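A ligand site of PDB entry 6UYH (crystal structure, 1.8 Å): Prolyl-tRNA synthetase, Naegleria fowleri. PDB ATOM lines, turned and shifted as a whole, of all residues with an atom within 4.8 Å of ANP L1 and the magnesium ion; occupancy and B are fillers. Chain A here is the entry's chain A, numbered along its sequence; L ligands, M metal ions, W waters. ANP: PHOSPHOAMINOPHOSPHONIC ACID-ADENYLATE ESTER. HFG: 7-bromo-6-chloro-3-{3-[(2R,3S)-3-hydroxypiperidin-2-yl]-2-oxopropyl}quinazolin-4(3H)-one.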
ATOM      1  N   GLU A  98       9.967   5.274  15.447  1.00  0.00           N
ATOM      2  CA  GLU A  98       9.929   4.941  14.025  1.00  0.00           C
ATOM      3  C   GLU A  98       8.520   4.930  13.430  1.00  0.00           C
ATOM      4  O   GLU A  98       8.383   4.727  12.222  1.00  0.00           O
ATOM      5  CB  GLU A  98      10.560   3.559  13.782  1.00  0.00           C
ATOM      6  CG  GLU A  98      12.051   3.468  14.071  1.00  0.00           C
ATOM      7  CD  GLU A  98      12.669   2.159  13.559  1.00  0.00           C
ATOM      8  OE1 GLU A  98      13.912   2.045  13.561  1.00  0.00           O
ATOM      9  OE2 GLU A  98      11.914   1.238  13.146  1.00  0.00           O
ATOM     10  N   ARG A 150       8.564   2.662   7.999  1.00  0.00           N
ATOM     11  CA  ARG A 150       9.294   2.855   9.258  1.00  0.00           C
ATOM     12  C   ARG A 150      10.172   4.083   9.124  1.00  0.00           C
ATOM     13  O   ARG A 150      10.953   4.185   8.175  1.00  0.00           O
ATOM     14  CB  ARG A 150      10.159   1.633   9.599  1.00  0.00           C
ATOM     15  CG  ARG A 150       9.381   0.348   9.784  1.00  0.00           C
ATOM     16  CD  ARG A 150      10.292  -0.869   9.875  1.00  0.00           C
ATOM     17  NE  ARG A 150       9.490  -2.083  10.028  1.00  0.00           N
ATOM     18  CZ  ARG A 150       9.998  -3.298  10.210  1.00  0.00           C
ATOM     19  NH1 ARG A 150      11.317  -3.469  10.269  1.00  0.00           N
ATOM     20  NH2 ARG A 150       9.198  -4.349  10.335  1.00  0.00           N
ATOM     21  N   GLU A 152      13.019   5.178   9.748  1.00  0.00           N
ATOM     22  CA  GLU A 152      14.334   4.685  10.136  1.00  0.00           C
ATOM     23  C   GLU A 152      15.223   5.813  10.620  1.00  0.00           C
ATOM     24  O   GLU A 152      15.334   6.860   9.983  1.00  0.00           O
ATOM     25  CB  GLU A 152      15.000   3.984   8.945  1.00  0.00           C
ATOM     26  CG  GLU A 152      14.211   2.798   8.356  1.00  0.00           C
ATOM     27  CD  GLU A 152      14.456   1.491   9.121  1.00  0.00           C
ATOM     28  OE1 GLU A 152      15.483   1.369   9.836  1.00  0.00           O
ATOM     29  OE2 GLU A 152      13.610   0.576   8.992  1.00  0.00           O
ATOM     30  N   LYS A 154      18.549   5.203  11.122  1.00  0.00           N
ATOM     31  CA  LYS A 154      19.771   4.993  10.359  1.00  0.00           C
ATOM     32  C   LYS A 154      19.671   5.634   8.967  1.00  0.00           C
ATOM     33  O   LYS A 154      18.583   5.799   8.425  1.00  0.00           O
ATOM     34  CB  LYS A 154      20.050   3.498  10.226  1.00  0.00           C
ATOM     35  CG  LYS A 154      20.428   2.802  11.531  1.00  0.00           C
ATOM     36  CD  LYS A 154      20.458   1.297  11.332  1.00  0.00           C
ATOM     37  CE  LYS A 154      20.958   0.576  12.574  1.00  0.00           C
ATOM     38  NZ  LYS A 154      20.937  -0.891  12.362  1.00  0.00           N
ATOM     39  N   PHE A 159      17.120   0.042  -1.507  1.00  0.00           N
ATOM     40  CA  PHE A 159      16.729  -1.348  -1.323  1.00  0.00           C
ATOM     41  C   PHE A 159      17.013  -1.886   0.077  1.00  0.00           C
ATOM     42  O   PHE A 159      16.115  -2.451   0.698  1.00  0.00           O
ATOM     43  CB  PHE A 159      17.389  -2.274  -2.363  1.00  0.00           C
ATOM     44  CG  PHE A 159      17.087  -1.909  -3.781  1.00  0.00           C
ATOM     45  CD1 PHE A 159      15.779  -1.921  -4.271  1.00  0.00           C
ATOM     46  CD2 PHE A 159      18.106  -1.557  -4.649  1.00  0.00           C
ATOM     47  CE1 PHE A 159      15.497  -1.575  -5.585  1.00  0.00           C
ATOM     48  CE2 PHE A 159      17.838  -1.216  -5.971  1.00  0.00           C
ATOM     49  CZ  PHE A 159      16.526  -1.232  -6.442  1.00  0.00           C
ATOM     50  N   ILE A 160      18.240  -1.703   0.596  1.00  0.00           N
ATOM     51  CA  ILE A 160      18.621  -2.358   1.846  1.00  0.00           C
ATOM     52  C   ILE A 160      17.848  -1.797   3.027  1.00  0.00           C
ATOM     53  O   ILE A 160      17.460  -2.529   3.941  1.00  0.00           O
ATOM     54  CB  ILE A 160      20.142  -2.221   2.095  1.00  0.00           C
ATOM     55  CG1 ILE A 160      20.943  -2.830   0.941  1.00  0.00           C
ATOM     56  CG2 ILE A 160      20.499  -2.856   3.449  1.00  0.00           C
ATOM     57  CD1 ILE A 160      20.792  -4.342   0.818  1.00  0.00           C
ATOM     58  N   ARG A 161      17.678  -0.467   3.065  1.00  0.00           N
ATOM     59  CA  ARG A 161      17.066   0.194   4.218  1.00  0.00           C
ATOM     60  C   ARG A 161      16.337   1.443   3.703  1.00  0.00           C
ATOM     61  O   ARG A 161      16.931   2.519   3.592  1.00  0.00           O
ATOM     62  CB  ARG A 161      18.101   0.560   5.275  1.00  0.00           C
ATOM     63  CG  ARG A 161      17.448   1.094   6.560  1.00  0.00           C
ATOM     64  CD  ARG A 161      18.463   1.428   7.648  1.00  0.00           C
ATOM     65  NE  ARG A 161      19.234   0.244   8.018  1.00  0.00           N
ATOM     66  CZ  ARG A 161      18.751  -0.784   8.694  1.00  0.00           C
ATOM     67  NH1 ARG A 161      17.484  -0.785   9.102  1.00  0.00           N
ATOM     68  NH2 ARG A 161      19.524  -1.828   8.979  1.00  0.00           N
ATOM     69  N   SER A 162      15.052   1.285   3.407  1.00  0.00           N
ATOM     70  CA  SER A 162      14.248   2.399   2.922  1.00  0.00           C
ATOM     71  C   SER A 162      13.118   2.675   3.905  1.00  0.00           C
ATOM     72  O   SER A 162      12.732   1.803   4.687  1.00  0.00           O
ATOM     73  CB  SER A 162      13.726   2.137   1.494  1.00  0.00           C
ATOM     74  OG  SER A 162      12.968   0.940   1.389  1.00  0.00           O
ATOM     75  N   PHE A 165       9.178   0.365   2.298  1.00  0.00           N
ATOM     76  CA  PHE A 165       9.676  -0.798   1.592  1.00  0.00           C
ATOM     77  C   PHE A 165       8.519  -1.748   1.337  1.00  0.00           C
ATOM     78  O   PHE A 165       7.399  -1.538   1.809  1.00  0.00           O
ATOM     79  CB  PHE A 165      10.848  -1.485   2.358  1.00  0.00           C
ATOM     80  CG  PHE A 165      10.526  -1.970   3.743  1.00  0.00           C
ATOM     81  CD1 PHE A 165      10.194  -3.301   3.963  1.00  0.00           C
ATOM     82  CD2 PHE A 165      10.638  -1.123   4.849  1.00  0.00           C
ATOM     83  CE1 PHE A 165       9.943  -3.780   5.240  1.00  0.00           C
ATOM     84  CE2 PHE A 165      10.391  -1.591   6.139  1.00  0.00           C
ATOM     85  CZ  PHE A 165      10.035  -2.927   6.331  1.00  0.00           C
ATOM     86  N   TRP A 167       7.255  -5.919   1.129  1.00  0.00           N
ATOM     87  CA  TRP A 167       7.603  -7.232   1.643  1.00  0.00           C
ATOM     88  C   TRP A 167       6.420  -8.169   1.469  1.00  0.00           C
ATOM     89  O   TRP A 167       5.359  -7.780   0.979  1.00  0.00           O
ATOM     90  CB  TRP A 167       8.065  -7.167   3.111  1.00  0.00           C
ATOM     91  CG  TRP A 167       7.002  -6.957   4.199  1.00  0.00           C
ATOM     92  CD1 TRP A 167       5.646  -6.796   4.047  1.00  0.00           C
ATOM     93  CD2 TRP A 167       7.266  -6.853   5.601  1.00  0.00           C
ATOM     94  NE1 TRP A 167       5.060  -6.628   5.292  1.00  0.00           N
ATOM     95  CE2 TRP A 167       6.033  -6.653   6.255  1.00  0.00           C
ATOM     96  CE3 TRP A 167       8.436  -6.924   6.369  1.00  0.00           C
ATOM     97  CZ2 TRP A 167       5.936  -6.519   7.639  1.00  0.00           C
ATOM     98  CZ3 TRP A 167       8.342  -6.789   7.742  1.00  0.00           C
ATOM     99  CH2 TRP A 167       7.096  -6.588   8.363  1.00  0.00           C
ATOM    100  N   LYS A 208      19.021 -15.981  15.760  1.00  0.00           N
ATOM    101  CA  LYS A 208      19.520 -14.741  16.329  1.00  0.00           C
ATOM    102  C   LYS A 208      19.739 -14.880  17.839  1.00  0.00           C
ATOM    103  O   LYS A 208      19.109 -15.703  18.516  1.00  0.00           O
ATOM    104  CB  LYS A 208      18.564 -13.588  16.038  1.00  0.00           C
ATOM    105  CG  LYS A 208      18.548 -13.176  14.587  1.00  0.00           C
ATOM    106  CD  LYS A 208      17.759 -11.898  14.420  1.00  0.00           C
ATOM    107  CE  LYS A 208      17.613 -11.538  12.950  1.00  0.00           C
ATOM    108  NZ  LYS A 208      16.861 -10.261  12.801  1.00  0.00           N
ATOM    109  N   GLN A 235      21.158  -8.930   6.952  1.00  0.00           N
ATOM    110  CA  GLN A 235      20.103  -9.805   7.423  1.00  0.00           C
ATOM    111  C   GLN A 235      19.058  -9.955   6.325  1.00  0.00           C
ATOM    112  O   GLN A 235      18.355  -8.999   5.995  1.00  0.00           O
ATOM    113  CB  GLN A 235      19.504  -9.242   8.715  1.00  0.00           C
ATOM    114  CG  GLN A 235      20.413  -9.410   9.949  1.00  0.00           C
ATOM    115  CD  GLN A 235      21.728  -8.620   9.881  1.00  0.00           C
ATOM    116  OE1 GLN A 235      21.725  -7.395   9.777  1.00  0.00           O
ATOM    117  NE2 GLN A 235      22.853  -9.335   9.943  1.00  0.00           N
ATOM    118  N   GLY A 236      18.972 -11.150   5.738  1.00  0.00           N
ATOM    119  CA  GLY A 236      18.285 -11.296   4.466  1.00  0.00           C
ATOM    120  C   GLY A 236      16.800 -11.622   4.531  1.00  0.00           C
ATOM    121  O   GLY A 236      16.126 -11.500   3.515  1.00  0.00           O
ATOM    122  N   GLY A 237      16.290 -12.022   5.685  1.00  0.00           N
ATOM    123  CA  GLY A 237      14.913 -12.448   5.815  1.00  0.00           C
ATOM    124  C   GLY A 237      14.763 -13.147   7.162  1.00  0.00           C
ATOM    125  O   GLY A 237      15.759 -13.599   7.720  1.00  0.00           O
ATOM    126  N   THR A 238      13.553 -13.230   7.689  1.00  0.00           N
ATOM    127  CA  THR A 238      13.398 -13.545   9.104  1.00  0.00           C
ATOM    128  C   THR A 238      12.227 -14.496   9.295  1.00  0.00           C
ATOM    129  O   THR A 238      11.171 -14.300   8.682  1.00  0.00           O
ATOM    130  CB  THR A 238      13.163 -12.263   9.901  1.00  0.00           C
ATOM    131  OG1 THR A 238      14.147 -11.289   9.539  1.00  0.00           O
ATOM    132  CG2 THR A 238      13.297 -12.541  11.364  1.00  0.00           C
ATOM    133  N   HIS A 240      10.177 -16.243  12.608  1.00  0.00           N
ATOM    134  CA  HIS A 240      10.034 -16.273  14.062  1.00  0.00           C
ATOM    135  C   HIS A 240       9.105 -17.386  14.491  1.00  0.00           C
ATOM    136  O   HIS A 240       8.037 -17.570  13.902  1.00  0.00           O
ATOM    137  CB  HIS A 240       9.422 -14.977  14.604  1.00  0.00           C
ATOM    138  CG  HIS A 240      10.088 -13.727  14.159  1.00  0.00           C
ATOM    139  ND1 HIS A 240      11.297 -13.305  14.681  1.00  0.00           N
ATOM    140  CD2 HIS A 240       9.693 -12.765  13.291  1.00  0.00           C
ATOM    141  CE1 HIS A 240      11.637 -12.160  14.123  1.00  0.00           C
ATOM    142  NE2 HIS A 240      10.673 -11.807  13.280  1.00  0.00           N
ATOM    143  N   GLY A 270       8.997 -12.730   7.383  1.00  0.00           N
ATOM    144  CA  GLY A 270       8.952 -11.704   6.353  1.00  0.00           C
ATOM    145  C   GLY A 270      10.216 -11.669   5.524  1.00  0.00           C
ATOM    146  O   GLY A 270      11.310 -11.971   5.998  1.00  0.00           O
ATOM    147  N   SER A 272      11.779  -8.960   2.232  1.00  0.00           N
ATOM    148  CA  SER A 272      11.500  -7.637   1.651  1.00  0.00           C
ATOM    149  C   SER A 272      12.305  -7.387   0.373  1.00  0.00           C
ATOM    150  O   SER A 272      13.147  -8.197  -0.041  1.00  0.00           O
ATOM    151  CB  SER A 272      11.833  -6.519   2.640  1.00  0.00           C
ATOM    152  OG  SER A 272      13.231  -6.296   2.651  1.00  0.00           O
ATOM    153  N   ARG A 274      14.726  -5.622   0.251  1.00  0.00           N
ATOM    154  CA  ARG A 274      16.144  -5.709   0.567  1.00  0.00           C
ATOM    155  C   ARG A 274      16.845  -6.751  -0.301  1.00  0.00           C
ATOM    156  O   ARG A 274      18.014  -6.576  -0.662  1.00  0.00           O
ATOM    157  CB  ARG A 274      16.304  -6.037   2.067  1.00  0.00           C
ATOM    158  CG  ARG A 274      17.702  -6.474   2.484  1.00  0.00           C
ATOM    159  CD  ARG A 274      17.798  -6.602   4.001  1.00  0.00           C
ATOM    160  NE  ARG A 274      17.630  -5.310   4.658  1.00  0.00           N
ATOM    161  CZ  ARG A 274      17.733  -5.120   5.960  1.00  0.00           C
ATOM    162  NH1 ARG A 274      18.032  -6.157   6.750  1.00  0.00           N
ATOM    163  NH2 ARG A 274      17.545  -3.912   6.470  1.00  0.00           N
ATOM    164  N   LYS A 474      28.568  -6.833  15.212  1.00  0.00           N
ATOM    165  CA  LYS A 474      27.383  -7.254  15.936  1.00  0.00           C
ATOM    166  C   LYS A 474      27.130  -8.728  15.674  1.00  0.00           C
ATOM    167  O   LYS A 474      27.749  -9.339  14.794  1.00  0.00           O
ATOM    168  CB  LYS A 474      26.172  -6.411  15.580  1.00  0.00           C
ATOM    169  CG  LYS A 474      25.668  -6.585  14.185  1.00  0.00           C
ATOM    170  CD  LYS A 474      24.538  -5.601  13.927  1.00  0.00           C
ATOM    171  CE  LYS A 474      23.209  -6.288  13.658  1.00  0.00           C
ATOM    172  NZ  LYS A 474      22.077  -5.317  13.814  1.00  0.00           N
HETATM  173  PG  ANP L   1      16.989  -4.474  10.637  1.00  0.00           P
HETATM  174  O1G ANP L   1      18.089  -4.551  11.587  1.00  0.00           O
HETATM  175  O2G ANP L   1      16.266  -3.075  10.843  1.00  0.00           O
HETATM  176  O3G ANP L   1      17.637  -4.596   9.197  1.00  0.00           O
HETATM  177  PB  ANP L   1      14.397  -5.712  11.478  1.00  0.00           P
HETATM  178  O1B ANP L   1      14.338  -6.452  12.732  1.00  0.00           O
HETATM  179  O2B ANP L   1      13.896  -4.253  11.712  1.00  0.00           O
HETATM  180  N3B ANP L   1      15.909  -5.691  10.825  1.00  0.00           N
HETATM  181  PA  ANP L   1      12.116  -7.157  10.433  1.00  0.00           P
HETATM  182  O1A ANP L   1      12.216  -8.442  11.151  1.00  0.00           O
HETATM  183  O2A ANP L   1      11.107  -6.265  11.090  1.00  0.00           O
HETATM  184  O3A ANP L   1      13.498  -6.370  10.400  1.00  0.00           O
HETATM  185  O5' ANP L   1      11.752  -7.252   8.876  1.00  0.00           O
HETATM  186  C5' ANP L   1      11.720  -8.438   8.042  1.00  0.00           C
HETATM  187  C4' ANP L   1      12.778  -8.273   6.998  1.00  0.00           C
HETATM  188  O4' ANP L   1      12.555  -7.057   6.251  1.00  0.00           O
HETATM  189  C3' ANP L   1      14.176  -8.105   7.581  1.00  0.00           C
HETATM  190  O3' ANP L   1      14.767  -9.375   7.833  1.00  0.00           O
HETATM  191  C2' ANP L   1      14.921  -7.345   6.478  1.00  0.00           C
HETATM  192  O2' ANP L   1      15.513  -8.256   5.552  1.00  0.00           O
HETATM  193  C1' ANP L   1      13.797  -6.500   5.838  1.00  0.00           C
HETATM  194  N9  ANP L   1      13.822  -5.097   6.225  1.00  0.00           N
HETATM  195  C8  ANP L   1      13.774  -4.580   7.489  1.00  0.00           C
HETATM  196  N7  ANP L   1      13.811  -3.278   7.545  1.00  0.00           N
HETATM  197  C5  ANP L   1      13.880  -2.896   6.210  1.00  0.00           C
HETATM  198  C6  ANP L   1      13.956  -1.639   5.587  1.00  0.00           C
HETATM  199  N6  ANP L   1      13.904  -0.478   6.242  1.00  0.00           N
HETATM  200  N1  ANP L   1      14.052  -1.617   4.235  1.00  0.00           N
HETATM  201  C2  ANP L   1      14.061  -2.770   3.573  1.00  0.00           C
HETATM  202  N3  ANP L   1      13.979  -4.020   4.050  1.00  0.00           N
HETATM  203  C4  ANP L   1      13.900  -4.013   5.390  1.00  0.00           C
HETATM  204  O4' HFG L   2       8.239  -6.655  12.212  1.00  0.00           O
HETATM  205  C21 HFG L   2       8.792  -7.288  13.086  1.00  0.00           C
HETATM  206  C3' HFG L   2       8.510  -8.752  13.310  1.00  0.00           C
HETATM  207  C2' HFG L   2       8.011  -9.532  12.084  1.00  0.00           C
HETATM  208  N1' HFG L   2       6.678  -9.101  11.637  1.00  0.00           N
HETATM  209  C6' HFG L   2       6.157  -9.952  10.569  1.00  0.00           C
HETATM  210  C5' HFG L   2       7.062  -9.955   9.364  1.00  0.00           C
HETATM  211  C4' HFG L   2       8.492 -10.336   9.758  1.00  0.00           C
HETATM  212  C39 HFG L   2       8.974  -9.466  10.905  1.00  0.00           C
HETATM  213  O7' HFG L   2      10.277  -9.902  11.313  1.00  0.00           O
HETATM  214  C1' HFG L   2       9.799  -6.619  14.033  1.00  0.00           C
HETATM  215  N3  HFG L   2       9.618  -5.167  14.095  1.00  0.00           N
HETATM  216  C4  HFG L   2       8.476  -4.699  14.719  1.00  0.00           C
HETATM  217  O11 HFG L   2       7.673  -5.452  15.237  1.00  0.00           O
HETATM  218  C10 HFG L   2       8.324  -3.231  14.654  1.00  0.00           C
HETATM  219  C5  HFG L   2       7.232  -2.613  15.246  1.00  0.00           C
HETATM  220  C2  HFG L   2      10.510  -4.340  13.485  1.00  0.00           C
HETATM  221  N1  HFG L   2      10.415  -3.061  13.383  1.00  0.00           N
HETATM  222  C9  HFG L   2       9.280  -2.478  13.970  1.00  0.00           C
HETATM  223  C8  HFG L   2       9.112  -1.102  13.830  1.00  0.00           C
HETATM  224  C7  HFG L   2       7.997  -0.500  14.404  1.00  0.00           C
HETATM  225 BR1  HFG L   2       7.741   1.345  14.113  1.00  0.00          BR
HETATM  226  C6  HFG L   2       7.091  -1.242  15.132  1.00  0.00           C
HETATM  227 CL1  HFG L   2       5.770  -0.479  15.967  1.00  0.00          CL
HETATM  228 MG    MG M   1      14.398  -2.306  11.854  1.00  0.00          MG
HETATM  229  O   HOH W   1      15.301  -2.671  13.912  1.00  0.00           O
HETATM  230  O   HOH W   2      15.156  -0.304  11.905  1.00  0.00           O
HETATM  231  O   HOH W   3      14.387  -9.342   3.368  1.00  0.00           O
HETATM  232  O   HOH W   4      12.911  -6.680  15.384  1.00  0.00           O
HETATM  233  O   HOH W   5      12.702  -1.657  12.762  1.00  0.00           O
HETATM  234  O   HOH W   6      18.741  -2.195  12.387  1.00  0.00           O
HETATM  235  O   HOH W   7      13.690  -1.807   9.918  1.00  0.00           O
HETATM  236  O   HOH W   8      12.610  -9.027  13.889  1.00  0.00           O
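Residues that only touch ANP L1: Ile 160, Phe 165, Phe 159, Trp 167, Gly 237 and Gly 236.
Hydrophobic or aromatic side chains that line ANP L1: Phe 165 and Trp 167.
Of the 20 residues printed, 14 come within 4 Å of ANP L1.
Along chain A the residues within 4 Å of ANP L1 span positions 150 to 274.
The nearest printed residue that does not touch ANP L1 is Gly 270 (4.1 Å).
The guanidinium group (NE) of Arg 274 sits at hydrogen-bond distance from the backbone carbonyl oxygen (O) of Ile 160, at 2.9 Å.
The side-chain carboxylate (OE1) of Glu 152 lies within salt-bridge range of the guanidinium group (NH1) of Arg 161.
The backbone carbonyl oxygen of Thr 238 sits at hydrogen-bond distance from the backbone NH of Gly 270, at 3.0 Å.
The backbone NH (N) of Arg 274 lies close to the backbone carbonyl oxygen (O) of Phe 159, at 3.5 Å.
OG of Ser 272 lies within hydrogen-bond range of N of Arg 274 (2.9 Å).
NH1 of Arg 274 lies within hydrogen-bond range of O of Gln 235 (3.0 Å).
N6 of ANP L1 is in hydrogen-bond range of O of Ser 162 (3.0 Å).
NH2 of Arg 150 lies within salt-bridge range of O2A of ANP L1 (2.8 Å).
OG1 of Thr 238 sits at hydrogen-bond distance from O3' of ANP L1 (2.6 Å).
An oxygen (O4') of HFG L2 is in hydrogen-bond range of the guanidinium group of Arg 150 (3.1 Å).
N3 of ANP L1 lies within hydrogen-bond range of OG of Ser 272 (2.8 Å).
A ring nitrogen (NE2) of His 240 lies within hydrogen-bond range of an oxygen (O7') of HFG L2, 2.8 Å away.
O2' of ANP L1 lies within hydrogen-bond range of O of Gln 235 (3.0 Å).
A nitrogen (N1) of ANP L1 lies within hydrogen-bond range of the backbone NH of Ser 162 (3.2 Å).
The side-chain carboxylate of Glu 152 lies within hydrogen-bond range of a nitrogen (N6) of ANP L1.
The guanidinium group (NH2) of Arg 274 lies within salt-bridge range of an oxygen (O3G) of ANP L1 (2.8 Å).
An oxygen (O3G) of ANP L1 lies within salt-bridge range of the guanidinium group (NH2) of Arg 161, 3.4 Å away.
An oxygen (O2B) of ANP L1 binds the magnesium ion.
The magnesium ion is bound by water W5, at 2.0 Å.
Water W7 binds the magnesium ion, at 2.1 Å.
The magnesium ion is bound by water W2, at 2.1 Å.
The magnesium ion is bound by O2G of ANP L1 (2.3 Å).
The magnesium ion is bound by water W1, at 2.3 Å.
NH1 of Arg 150 touches the magnesium ion (3.7 Å).
Of the 20 residues printed, 1 comes within 4 Å of the magnesium ion.
Water W2 bridges the side-chain carboxylate of Glu 152 and the side-chain carboxylate of Glu 98.
Water W5 lies within hydrogen-bond range of a nitrogen (N1) of HFG L2, the side-chain carboxylate (OE2) of Glu 98 and the guanidinium group (NH1) of Arg 150.
Water W7 lies within hydrogen-bond range of OE2 of Glu 152 (2.6 Å), N7 of ANP L1 (2.8 Å) and NH1 of Arg 150 (2.9 Å).
Water W6 bridges NZ of Lys 154 (2.6 Å) and O1G of ANP L1 (2.6 Å).
Water W3 lies within hydrogen-bond range of an oxygen (O2') of ANP L1 (2.7 Å), the backbone carbonyl oxygen (O) of Gly 236 (2.8 Å) and the backbone NH (N) of Ser 272 (2.9 Å).
Water W8 lies within hydrogen-bond range of an oxygen (O1A) of ANP L1 and a ring nitrogen (NE2) of His 240.
An oxygen (O7') of HFG L2 is in hydrogen-bond range of an oxygen (O1A) of ANP L1 (2.4 Å).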
